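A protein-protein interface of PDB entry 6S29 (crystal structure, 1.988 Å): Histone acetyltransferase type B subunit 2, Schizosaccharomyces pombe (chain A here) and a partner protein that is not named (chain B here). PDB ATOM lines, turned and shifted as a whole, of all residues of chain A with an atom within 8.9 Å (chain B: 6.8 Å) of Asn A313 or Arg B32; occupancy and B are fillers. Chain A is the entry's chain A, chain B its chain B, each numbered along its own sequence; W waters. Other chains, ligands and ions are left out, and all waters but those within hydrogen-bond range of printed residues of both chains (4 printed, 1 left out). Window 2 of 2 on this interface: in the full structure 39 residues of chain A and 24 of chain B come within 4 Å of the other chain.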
ATOM      1  N   LYS A 275      17.155   6.904  -9.304  1.00  0.00           N
ATOM      2  CA  LYS A 275      17.492   8.281  -8.976  1.00  0.00           C
ATOM      3  C   LYS A 275      18.266   8.942 -10.117  1.00  0.00           C
ATOM      4  O   LYS A 275      19.235   8.384 -10.645  1.00  0.00           O
ATOM      5  CB  LYS A 275      18.285   8.367  -7.651  1.00  0.00           C
ATOM      6  CG  LYS A 275      17.761   7.463  -6.522  1.00  0.00           C
ATOM      7  CD  LYS A 275      18.240   7.849  -5.130  1.00  0.00           C
ATOM      8  CE  LYS A 275      19.733   7.613  -5.000  1.00  0.00           C
ATOM      9  NZ  LYS A 275      20.281   8.127  -3.715  1.00  0.00           N
ATOM     10  N   ILE A 277      20.086  12.618 -10.874  1.00  0.00           N
ATOM     11  CA  ILE A 277      20.591  13.797 -10.174  1.00  0.00           C
ATOM     12  C   ILE A 277      21.090  14.792 -11.213  1.00  0.00           C
ATOM     13  O   ILE A 277      21.969  14.466 -12.023  1.00  0.00           O
ATOM     14  CB  ILE A 277      21.695  13.429  -9.165  1.00  0.00           C
ATOM     15  CG1 ILE A 277      21.106  12.546  -8.050  1.00  0.00           C
ATOM     16  CG2 ILE A 277      22.341  14.686  -8.589  1.00  0.00           C
ATOM     17  CD1 ILE A 277      22.106  11.632  -7.360  1.00  0.00           C
ATOM     18  N   TYR A 295      28.844   6.388   1.329  1.00  0.00           N
ATOM     19  CA  TYR A 295      27.869   7.343   0.821  1.00  0.00           C
ATOM     20  C   TYR A 295      28.511   8.513   0.086  1.00  0.00           C
ATOM     21  O   TYR A 295      27.799   9.406  -0.397  1.00  0.00           O
ATOM     22  CB  TYR A 295      27.012   7.855   1.987  1.00  0.00           C
ATOM     23  CG  TYR A 295      26.281   6.716   2.654  1.00  0.00           C
ATOM     24  CD1 TYR A 295      25.380   5.953   1.934  1.00  0.00           C
ATOM     25  CD2 TYR A 295      26.536   6.372   3.970  1.00  0.00           C
ATOM     26  CE1 TYR A 295      24.707   4.898   2.520  1.00  0.00           C
ATOM     27  CE2 TYR A 295      25.874   5.310   4.568  1.00  0.00           C
ATOM     28  CZ  TYR A 295      24.967   4.581   3.829  1.00  0.00           C
ATOM     29  OH  TYR A 295      24.299   3.528   4.398  1.00  0.00           O
ATOM     30  N   LEU A 308      30.935  17.063  -4.708  1.00  0.00           N
ATOM     31  CA  LEU A 308      30.863  15.948  -3.773  1.00  0.00           C
ATOM     32  C   LEU A 308      29.417  15.724  -3.347  1.00  0.00           C
ATOM     33  O   LEU A 308      28.656  16.679  -3.179  1.00  0.00           O
ATOM     34  CB  LEU A 308      31.728  16.213  -2.540  1.00  0.00           C
ATOM     35  CG  LEU A 308      33.195  16.542  -2.802  1.00  0.00           C
ATOM     36  CD1 LEU A 308      33.888  16.903  -1.495  1.00  0.00           C
ATOM     37  CD2 LEU A 308      33.861  15.347  -3.467  1.00  0.00           C
ATOM     38  N   TRP A 309      29.056  14.466  -3.107  1.00  0.00           N
ATOM     39  CA  TRP A 309      27.657  14.099  -2.895  1.00  0.00           C
ATOM     40  C   TRP A 309      27.546  13.070  -1.784  1.00  0.00           C
ATOM     41  O   TRP A 309      28.419  12.214  -1.622  1.00  0.00           O
ATOM     42  CB  TRP A 309      27.010  13.515  -4.174  1.00  0.00           C
ATOM     43  CG  TRP A 309      27.158  14.430  -5.363  1.00  0.00           C
ATOM     44  CD1 TRP A 309      28.213  14.469  -6.239  1.00  0.00           C
ATOM     45  CD2 TRP A 309      26.251  15.457  -5.779  1.00  0.00           C
ATOM     46  NE1 TRP A 309      28.002  15.454  -7.194  1.00  0.00           N
ATOM     47  CE2 TRP A 309      26.812  16.078  -6.927  1.00  0.00           C
ATOM     48  CE3 TRP A 309      25.013  15.905  -5.309  1.00  0.00           C
ATOM     49  CZ2 TRP A 309      26.183  17.123  -7.594  1.00  0.00           C
ATOM     50  CZ3 TRP A 309      24.379  16.943  -5.982  1.00  0.00           C
ATOM     51  CH2 TRP A 309      24.969  17.544  -7.110  1.00  0.00           C
ATOM     52  N   ASP A 310      26.453  13.164  -1.027  1.00  0.00           N
ATOM     53  CA  ASP A 310      26.018  12.121  -0.098  1.00  0.00           C
ATOM     54  C   ASP A 310      24.871  11.387  -0.778  1.00  0.00           C
ATOM     55  O   ASP A 310      23.810  11.980  -1.022  1.00  0.00           O
ATOM     56  CB  ASP A 310      25.573  12.738   1.230  1.00  0.00           C
ATOM     57  CG  ASP A 310      25.033  11.705   2.248  1.00  0.00           C
ATOM     58  OD1 ASP A 310      24.693  10.559   1.892  1.00  0.00           O
ATOM     59  OD2 ASP A 310      24.957  12.063   3.435  1.00  0.00           O
ATOM     60  N   LEU A 311      25.089  10.108  -1.096  1.00  0.00           N
ATOM     61  CA  LEU A 311      24.069   9.321  -1.787  1.00  0.00           C
ATOM     62  C   LEU A 311      22.760   9.244  -1.016  1.00  0.00           C
ATOM     63  O   LEU A 311      21.721   8.976  -1.624  1.00  0.00           O
ATOM     64  CB  LEU A 311      24.558   7.894  -2.050  1.00  0.00           C
ATOM     65  CG  LEU A 311      25.332   7.771  -3.360  1.00  0.00           C
ATOM     66  CD1 LEU A 311      26.240   6.543  -3.323  1.00  0.00           C
ATOM     67  CD2 LEU A 311      24.388   7.723  -4.535  1.00  0.00           C
ATOM     68  N   ARG A 312      22.788   9.420   0.303  1.00  0.00           N
ATOM     69  CA  ARG A 312      21.550   9.406   1.069  1.00  0.00           C
ATOM     70  C   ARG A 312      20.775  10.694   0.921  1.00  0.00           C
ATOM     71  O   ARG A 312      19.567  10.702   1.135  1.00  0.00           O
ATOM     72  CB  ARG A 312      21.822   9.191   2.556  1.00  0.00           C
ATOM     73  CG  ARG A 312      22.512   7.884   2.882  1.00  0.00           C
ATOM     74  CD  ARG A 312      23.187   7.988   4.250  1.00  0.00           C
ATOM     75  NE  ARG A 312      24.075   9.148   4.351  1.00  0.00           N
ATOM     76  CZ  ARG A 312      24.865   9.373   5.399  1.00  0.00           C
ATOM     77  NH1 ARG A 312      24.858   8.520   6.414  1.00  0.00           N
ATOM     78  NH2 ARG A 312      25.662  10.439   5.440  1.00  0.00           N
ATOM     79  N   ASN A 313      21.447  11.784   0.591  1.00  0.00           N
ATOM     80  CA  ASN A 313      20.821  13.093   0.449  1.00  0.00           C
ATOM     81  C   ASN A 313      21.270  13.623  -0.904  1.00  0.00           C
ATOM     82  O   ASN A 313      22.069  14.558  -0.993  1.00  0.00           O
ATOM     83  CB  ASN A 313      21.211  13.994   1.622  1.00  0.00           C
ATOM     84  CG  ASN A 313      20.817  13.386   2.980  1.00  0.00           C
ATOM     85  OD1 ASN A 313      19.657  13.492   3.397  1.00  0.00           O
ATOM     86  ND2 ASN A 313      21.774  12.712   3.654  1.00  0.00           N
ATOM     87  N   PRO A 314      20.742  13.042  -1.984  1.00  0.00           N
ATOM     88  CA  PRO A 314      21.449  13.042  -3.271  1.00  0.00           C
ATOM     89  C   PRO A 314      21.205  14.229  -4.175  1.00  0.00           C
ATOM     90  O   PRO A 314      21.965  14.429  -5.131  1.00  0.00           O
ATOM     91  CB  PRO A 314      20.925  11.767  -3.945  1.00  0.00           C
ATOM     92  CG  PRO A 314      19.578  11.503  -3.316  1.00  0.00           C
ATOM     93  CD  PRO A 314      19.456  12.324  -2.056  1.00  0.00           C
ATOM     94  N   TYR A 315      20.164  15.011  -3.931  1.00  0.00           N
ATOM     95  CA  TYR A 315      19.897  16.127  -4.816  1.00  0.00           C
ATOM     96  C   TYR A 315      20.466  17.421  -4.271  1.00  0.00           C
ATOM     97  O   TYR A 315      20.230  18.488  -4.853  1.00  0.00           O
ATOM     98  CB  TYR A 315      18.400  16.296  -5.068  1.00  0.00           C
ATOM     99  CG  TYR A 315      17.766  15.034  -5.544  1.00  0.00           C
ATOM    100  CD1 TYR A 315      16.869  14.337  -4.740  1.00  0.00           C
ATOM    101  CD2 TYR A 315      18.090  14.508  -6.791  1.00  0.00           C
ATOM    102  CE1 TYR A 315      16.290  13.148  -5.179  1.00  0.00           C
ATOM    103  CE2 TYR A 315      17.526  13.327  -7.242  1.00  0.00           C
ATOM    104  CZ  TYR A 315      16.624  12.642  -6.434  1.00  0.00           C
ATOM    105  OH  TYR A 315      16.065  11.454  -6.881  1.00  0.00           O
ATOM    106  N   GLN A 316      21.219  17.363  -3.172  1.00  0.00           N
ATOM    107  CA  GLN A 316      21.851  18.572  -2.660  1.00  0.00           C
ATOM    108  C   GLN A 316      23.339  18.362  -2.383  1.00  0.00           C
ATOM    109  O   GLN A 316      23.732  17.714  -1.408  1.00  0.00           O
ATOM    110  CB  GLN A 316      21.063  19.143  -1.496  1.00  0.00           C
ATOM    111  CG  GLN A 316      19.991  19.963  -2.208  1.00  0.00           C
ATOM    112  CD  GLN A 316      19.644  21.252  -1.507  1.00  0.00           C
ATOM    113  OE1 GLN A 316      20.215  22.299  -1.805  1.00  0.00           O
ATOM    114  NE2 GLN A 316      18.589  21.214  -0.696  1.00  0.00           N
ATOM    115  N   ARG A 317      24.147  18.972  -3.243  1.00  0.00           N
ATOM    116  CA  ARG A 317      25.591  18.830  -3.255  1.00  0.00           C
ATOM    117  C   ARG A 317      26.208  19.120  -1.892  1.00  0.00           C
ATOM    118  O   ARG A 317      25.831  20.083  -1.218  1.00  0.00           O
ATOM    119  CB  ARG A 317      26.093  19.806  -4.330  1.00  0.00           C
ATOM    120  CG  ARG A 317      27.534  19.987  -4.491  1.00  0.00           C
ATOM    121  CD  ARG A 317      27.765  21.210  -5.400  1.00  0.00           C
ATOM    122  NE  ARG A 317      27.212  21.030  -6.751  1.00  0.00           N
ATOM    123  CZ  ARG A 317      27.737  21.605  -7.835  1.00  0.00           C
ATOM    124  NH1 ARG A 317      28.815  22.381  -7.712  1.00  0.00           N
ATOM    125  NH2 ARG A 317      27.208  21.412  -9.037  1.00  0.00           N
ATOM    126  N   LEU A 318      27.147  18.259  -1.479  1.00  0.00           N
ATOM    127  CA  LEU A 318      27.869  18.456  -0.225  1.00  0.00           C
ATOM    128  C   LEU A 318      28.814  19.652  -0.284  1.00  0.00           C
ATOM    129  O   LEU A 318      28.969  20.370   0.710  1.00  0.00           O
ATOM    130  CB  LEU A 318      28.711  17.228   0.096  1.00  0.00           C
ATOM    131  CG  LEU A 318      28.092  16.001   0.711  1.00  0.00           C
ATOM    132  CD1 LEU A 318      29.226  15.007   0.922  1.00  0.00           C
ATOM    133  CD2 LEU A 318      27.410  16.383   2.015  1.00  0.00           C
ATOM    134  N   HIS A 319      29.524  19.825  -1.400  1.00  0.00           N
ATOM    135  CA  HIS A 319      30.638  20.770  -1.491  1.00  0.00           C
ATOM    136  C   HIS A 319      31.068  20.846  -2.948  1.00  0.00           C
ATOM    137  O   HIS A 319      30.792  19.940  -3.743  1.00  0.00           O
ATOM    138  CB  HIS A 319      31.822  20.339  -0.601  1.00  0.00           C
ATOM    139  CG  HIS A 319      32.981  21.293  -0.615  1.00  0.00           C
ATOM    140  ND1 HIS A 319      32.903  22.572  -0.108  1.00  0.00           N
ATOM    141  CD2 HIS A 319      34.243  21.156  -1.088  1.00  0.00           C
ATOM    142  CE1 HIS A 319      34.070  23.175  -0.245  1.00  0.00           C
ATOM    143  NE2 HIS A 319      34.904  22.336  -0.837  1.00  0.00           N
ATOM    144  N   THR A 320      31.746  21.936  -3.295  1.00  0.00           N
ATOM    145  CA  THR A 320      32.279  22.134  -4.637  1.00  0.00           C
ATOM    146  C   THR A 320      33.780  22.355  -4.535  1.00  0.00           C
ATOM    147  O   THR A 320      34.230  23.262  -3.824  1.00  0.00           O
ATOM    148  CB  THR A 320      31.626  23.329  -5.327  1.00  0.00           C
ATOM    149  OG1 THR A 320      30.212  23.134  -5.407  1.00  0.00           O
ATOM    150  CG2 THR A 320      32.175  23.472  -6.741  1.00  0.00           C
ATOM    151  N   LEU A 355      39.934  16.551   1.751  1.00  0.00           N
ATOM    152  CA  LEU A 355      38.608  16.935   2.243  1.00  0.00           C
ATOM    153  C   LEU A 355      38.627  17.403   3.694  1.00  0.00           C
ATOM    154  O   LEU A 355      37.791  18.226   4.080  1.00  0.00           O
ATOM    155  CB  LEU A 355      37.632  15.771   2.088  1.00  0.00           C
ATOM    156  CG  LEU A 355      36.845  15.790   0.771  1.00  0.00           C
ATOM    157  CD1 LEU A 355      37.793  15.730  -0.419  1.00  0.00           C
ATOM    158  CD2 LEU A 355      35.861  14.654   0.708  1.00  0.00           C
ATOM    159  N   ILE A 358      38.567  21.236   4.278  1.00  0.00           N
ATOM    160  CA  ILE A 358      37.450  22.044   3.807  1.00  0.00           C
ATOM    161  C   ILE A 358      36.983  22.972   4.914  1.00  0.00           C
ATOM    162  O   ILE A 358      36.787  22.552   6.063  1.00  0.00           O
ATOM    163  CB  ILE A 358      36.312  21.145   3.303  1.00  0.00           C
ATOM    164  CG1 ILE A 358      36.641  20.640   1.908  1.00  0.00           C
ATOM    165  CG2 ILE A 358      34.965  21.894   3.278  1.00  0.00           C
ATOM    166  CD1 ILE A 358      35.734  19.520   1.449  1.00  0.00           C
ATOM    167  N   GLY A 359      36.857  24.259   4.579  1.00  0.00           N
ATOM    168  CA  GLY A 359      36.318  25.251   5.489  1.00  0.00           C
ATOM    169  C   GLY A 359      37.318  25.935   6.391  1.00  0.00           C
ATOM    170  O   GLY A 359      36.917  26.800   7.182  1.00  0.00           O
ATOM    171  N   ASN B  27      32.668  12.654   8.552  1.00  0.00           N
ATOM    172  CA  ASN B  27      31.234  12.784   8.750  1.00  0.00           C
ATOM    173  C   ASN B  27      30.672  13.731   7.688  1.00  0.00           C
ATOM    174  O   ASN B  27      31.028  14.915   7.651  1.00  0.00           O
ATOM    175  CB  ASN B  27      30.914  13.279  10.156  1.00  0.00           C
ATOM    176  CG  ASN B  27      29.447  13.243  10.424  1.00  0.00           C
ATOM    177  OD1 ASN B  27      28.711  14.096   9.933  1.00  0.00           O
ATOM    178  ND2 ASN B  27      28.986  12.217  11.147  1.00  0.00           N
ATOM    179  N   LEU B  28      29.781  13.212   6.835  1.00  0.00           N
ATOM    180  CA  LEU B  28      29.307  14.005   5.697  1.00  0.00           C
ATOM    181  C   LEU B  28      28.405  15.144   6.138  1.00  0.00           C
ATOM    182  O   LEU B  28      28.406  16.205   5.507  1.00  0.00           O
ATOM    183  CB  LEU B  28      28.561  13.117   4.687  1.00  0.00           C
ATOM    184  CG  LEU B  28      29.345  11.937   4.086  1.00  0.00           C
ATOM    185  CD1 LEU B  28      28.568  11.296   2.928  1.00  0.00           C
ATOM    186  CD2 LEU B  28      30.733  12.400   3.616  1.00  0.00           C
ATOM    187  N   HIS B  29      27.638  14.952   7.220  1.00  0.00           N
ATOM    188  CA  HIS B  29      26.821  16.040   7.746  1.00  0.00           C
ATOM    189  C   HIS B  29      27.698  17.161   8.277  1.00  0.00           C
ATOM    190  O   HIS B  29      27.359  18.343   8.128  1.00  0.00           O
ATOM    191  CB  HIS B  29      25.888  15.522   8.859  1.00  0.00           C
ATOM    192  CG  HIS B  29      25.074  14.333   8.452  1.00  0.00           C
ATOM    193  ND1 HIS B  29      24.274  14.333   7.329  1.00  0.00           N
ATOM    194  CD2 HIS B  29      24.962  13.094   8.996  1.00  0.00           C
ATOM    195  CE1 HIS B  29      23.692  13.151   7.207  1.00  0.00           C
ATOM    196  NE2 HIS B  29      24.097  12.378   8.199  1.00  0.00           N
ATOM    197  N   SER B  30      28.820  16.818   8.916  1.00  0.00           N
ATOM    198  CA  SER B  30      29.735  17.863   9.368  1.00  0.00           C
ATOM    199  C   SER B  30      30.410  18.565   8.196  1.00  0.00           C
ATOM    200  O   SER B  30      30.541  19.796   8.195  1.00  0.00           O
ATOM    201  CB  SER B  30      30.784  17.270  10.321  1.00  0.00           C
ATOM    202  OG  SER B  30      31.749  18.268  10.639  1.00  0.00           O
ATOM    203  N   LEU B  31      30.823  17.802   7.178  1.00  0.00           N
ATOM    204  CA  LEU B  31      31.407  18.423   5.983  1.00  0.00           C
ATOM    205  C   LEU B  31      30.425  19.384   5.309  1.00  0.00           C
ATOM    206  O   LEU B  31      30.811  20.472   4.856  1.00  0.00           O
ATOM    207  CB  LEU B  31      31.847  17.346   4.990  1.00  0.00           C
ATOM    208  CG  LEU B  31      32.652  17.786   3.755  1.00  0.00           C
ATOM    209  CD1 LEU B  31      33.594  16.683   3.314  1.00  0.00           C
ATOM    210  CD2 LEU B  31      31.747  18.149   2.599  1.00  0.00           C
ATOM    211  N   ARG B  32      29.151  18.991   5.202  1.00  0.00           N
ATOM    212  CA  ARG B  32      28.170  19.863   4.556  1.00  0.00           C
ATOM    213  C   ARG B  32      28.033  21.190   5.308  1.00  0.00           C
ATOM    214  O   ARG B  32      28.065  22.270   4.704  1.00  0.00           O
ATOM    215  CB  ARG B  32      26.815  19.140   4.457  1.00  0.00           C
ATOM    216  CG  ARG B  32      25.745  19.900   3.672  1.00  0.00           C
ATOM    217  CD  ARG B  32      24.341  19.336   3.926  1.00  0.00           C
ATOM    218  NE  ARG B  32      24.216  17.931   3.541  1.00  0.00           N
ATOM    219  CZ  ARG B  32      24.003  17.535   2.294  1.00  0.00           C
ATOM    220  NH1 ARG B  32      23.899  18.436   1.319  1.00  0.00           N
ATOM    221  NH2 ARG B  32      23.890  16.251   2.019  1.00  0.00           N
ATOM    222  N   SER B  33      27.908  21.139   6.640  1.00  0.00           N
ATOM    223  CA  SER B  33      27.772  22.387   7.392  1.00  0.00           C
ATOM    224  C   SER B  33      29.034  23.242   7.310  1.00  0.00           C
ATOM    225  O   SER B  33      28.943  24.468   7.178  1.00  0.00           O
ATOM    226  CB  SER B  33      27.422  22.100   8.848  1.00  0.00           C
ATOM    227  OG  SER B  33      28.542  21.561   9.508  1.00  0.00           O
ATOM    228  N   LYS B  34      30.219  22.628   7.422  1.00  0.00           N
ATOM    229  CA  LYS B  34      31.456  23.404   7.285  1.00  0.00           C
ATOM    230  C   LYS B  34      31.560  24.058   5.917  1.00  0.00           C
ATOM    231  O   LYS B  34      31.996  25.208   5.805  1.00  0.00           O
ATOM    232  CB  LYS B  34      32.678  22.536   7.568  1.00  0.00           C
ATOM    233  CG  LYS B  34      33.068  22.626   9.022  1.00  0.00           C
ATOM    234  CD  LYS B  34      34.001  21.522   9.486  1.00  0.00           C
ATOM    235  CE  LYS B  34      34.677  20.850   8.337  1.00  0.00           C
ATOM    236  NZ  LYS B  34      35.461  19.678   8.825  1.00  0.00           N
ATOM    237  N   SER B  35      31.191  23.338   4.861  1.00  0.00           N
ATOM    238  CA  SER B  35      31.182  23.958   3.546  1.00  0.00           C
ATOM    239  C   SER B  35      30.268  25.183   3.524  1.00  0.00           C
ATOM    240  O   SER B  35      30.648  26.247   3.019  1.00  0.00           O
ATOM    241  CB  SER B  35      30.767  22.954   2.480  1.00  0.00           C
ATOM    242  OG  SER B  35      30.671  23.591   1.211  1.00  0.00           O
ATOM    243  N   LEU B  36      29.035  25.046   4.034  1.00  0.00           N
ATOM    244  CA  LEU B  36      28.056  26.128   3.908  1.00  0.00           C
ATOM    245  C   LEU B  36      28.416  27.303   4.789  1.00  0.00           C
ATOM    246  O   LEU B  36      28.197  28.454   4.406  1.00  0.00           O
ATOM    247  CB  LEU B  36      26.651  25.633   4.264  1.00  0.00           C
ATOM    248  CG  LEU B  36      26.029  24.698   3.235  1.00  0.00           C
ATOM    249  CD1 LEU B  36      24.908  23.896   3.893  1.00  0.00           C
ATOM    250  CD2 LEU B  36      25.527  25.466   1.985  1.00  0.00           C
ATOM    251  N   ILE B  37      28.925  27.022   5.988  1.00  0.00           N
ATOM    252  CA  ILE B  37      29.273  28.065   6.941  1.00  0.00           C
ATOM    253  C   ILE B  37      30.491  28.838   6.460  1.00  0.00           C
ATOM    254  O   ILE B  37      30.550  30.074   6.572  1.00  0.00           O
ATOM    255  CB  ILE B  37      29.498  27.438   8.328  1.00  0.00           C
ATOM    256  CG1 ILE B  37      28.157  26.925   8.898  1.00  0.00           C
ATOM    257  CG2 ILE B  37      30.166  28.430   9.271  1.00  0.00           C
ATOM    258  CD1 ILE B  37      28.305  26.187  10.223  1.00  0.00           C
HETATM  259  O   HOH W   1      24.630  15.254  -1.211  1.00  0.00           O
HETATM  260  O   HOH W   2      24.956  14.651   4.030  1.00  0.00           O
HETATM  261  O   HOH W   3      36.101  18.989   6.357  1.00  0.00           O
HETATM  262  O   HOH W   4      31.244  24.726  -1.977  1.00  0.00           O
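Of the printed residues of chain B, Asp A310 touches Leu B28 and Arg B32. Of chain B, only Arg B32 (3.5 Å) comes within 4 Å of Asn A313. Tyr A315 touches none of the printed residues of chain B. Printed residues of chain B within 4 Å of Leu A318: Leu B28 (3.6 Å), Arg B32 (3.5 Å) and Ser B35 (3.6 Å). Of the printed residues of chain B, His A319 touches Leu B31 (3.9 Å) and Ser B35 (2.8 Å). Of chain A, only Asp A310, Asn A313, Gln A316, Arg A317 and Leu A318 come within 4 Å of Arg B32. No residue of chain A comes within 4 Å of Ser B33. The nearest residue of chain A that does not touch Arg B32 is Pro A314 (6.0 Å).
The backbone carbonyl oxygen (O) of Gln A316 lies within hydrogen-bond range of the guanidinium group (NH1) of Arg B32 (2.8 Å). The side-chain hydroxyl of Ser B35 lies within hydrogen-bond range of a ring nitrogen (ND1) of His A319, at 2.8 Å.
Of the 11 printed residues of chain B, 6 touch a printed residue of chain A. Along chain B the printed residues that touch a printed residue of chain A span positions 28 to 35. Of the 19 printed residues of chain A, 9 touch a printed residue of chain B. Hydrophobic or aromatic side chains of chain A that line the printed part of chain B: Tyr A295, Leu A318 and His A319. Along chain A the printed residues that touch a printed residue of chain B span positions 295 to 358. Among the printed residues, 14 pairs touch across the chains.
O of Tyr A295 is in hydrogen-bond range of N of Leu A311 (2.9 Å). The backbone carbonyl oxygen (O) of Leu A308 is in hydrogen-bond range of the backbone NH (N) of Leu A318. The backbone NH (N) of Leu A308 sits at hydrogen-bond distance from the backbone carbonyl oxygen (O) of His A319. OD2 of Asp A310 lies within salt-bridge range of NH2 of Arg A312, 2.7 Å away. OD2 of Asp A310 lies within hydrogen-bond range of ND2 of Asn A313, at 3.3 Å. The backbone NH (N) of His B29 lies within hydrogen-bond range of the side-chain amide oxygen (OD1) of Asn B27 (3.0 Å).
Water W1 lies within hydrogen-bond range of the backbone carbonyl oxygen of Gln A316, the backbone carbonyl oxygen of Asn A313, the backbone NH of Asp A310 and the guanidinium group of Arg B32. Water W3 lies within hydrogen-bond range of the side-chain amino group of Lys B34 (2.6 Å) and the backbone carbonyl oxygen of Leu A355 (2.9 Å). Water W2 lies within hydrogen-bond range of the side-chain carboxylate of Asp A310 (2.7 Å), the guanidinium group of Arg B32 (2.8 Å) and a ring nitrogen (ND1) of His B29 (3.4 Å). Water W4 lies within hydrogen-bond range of N of Thr A320 (3.1 Å), ND1 of His A319 (3.3 Å) and OG of Ser B35 (3.4 Å).
Among the printed residues, merely in contact across the chains: Tyr A295 with Leu B28 (3.9 Å), Asp A310 with Leu B28 (3.6 Å), Asp A310 with Arg B32 (3.97 Å), Arg A312 with Leu B28 (3.9 Å), Arg A312 with His B29 (3.7 Å), Asn A313 with Arg B32 (3.5 Å), Arg A317 with Arg B32 (3.6 Å), Leu A318 with Leu B28 (3.6 Å), Leu A318 with Arg B32 (3.5 Å), Leu A318 with Ser B35 (3.6 Å), His A319 with Leu B31 (3.9 Å) and Ile A358 with Lys B34 (3.5 Å).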
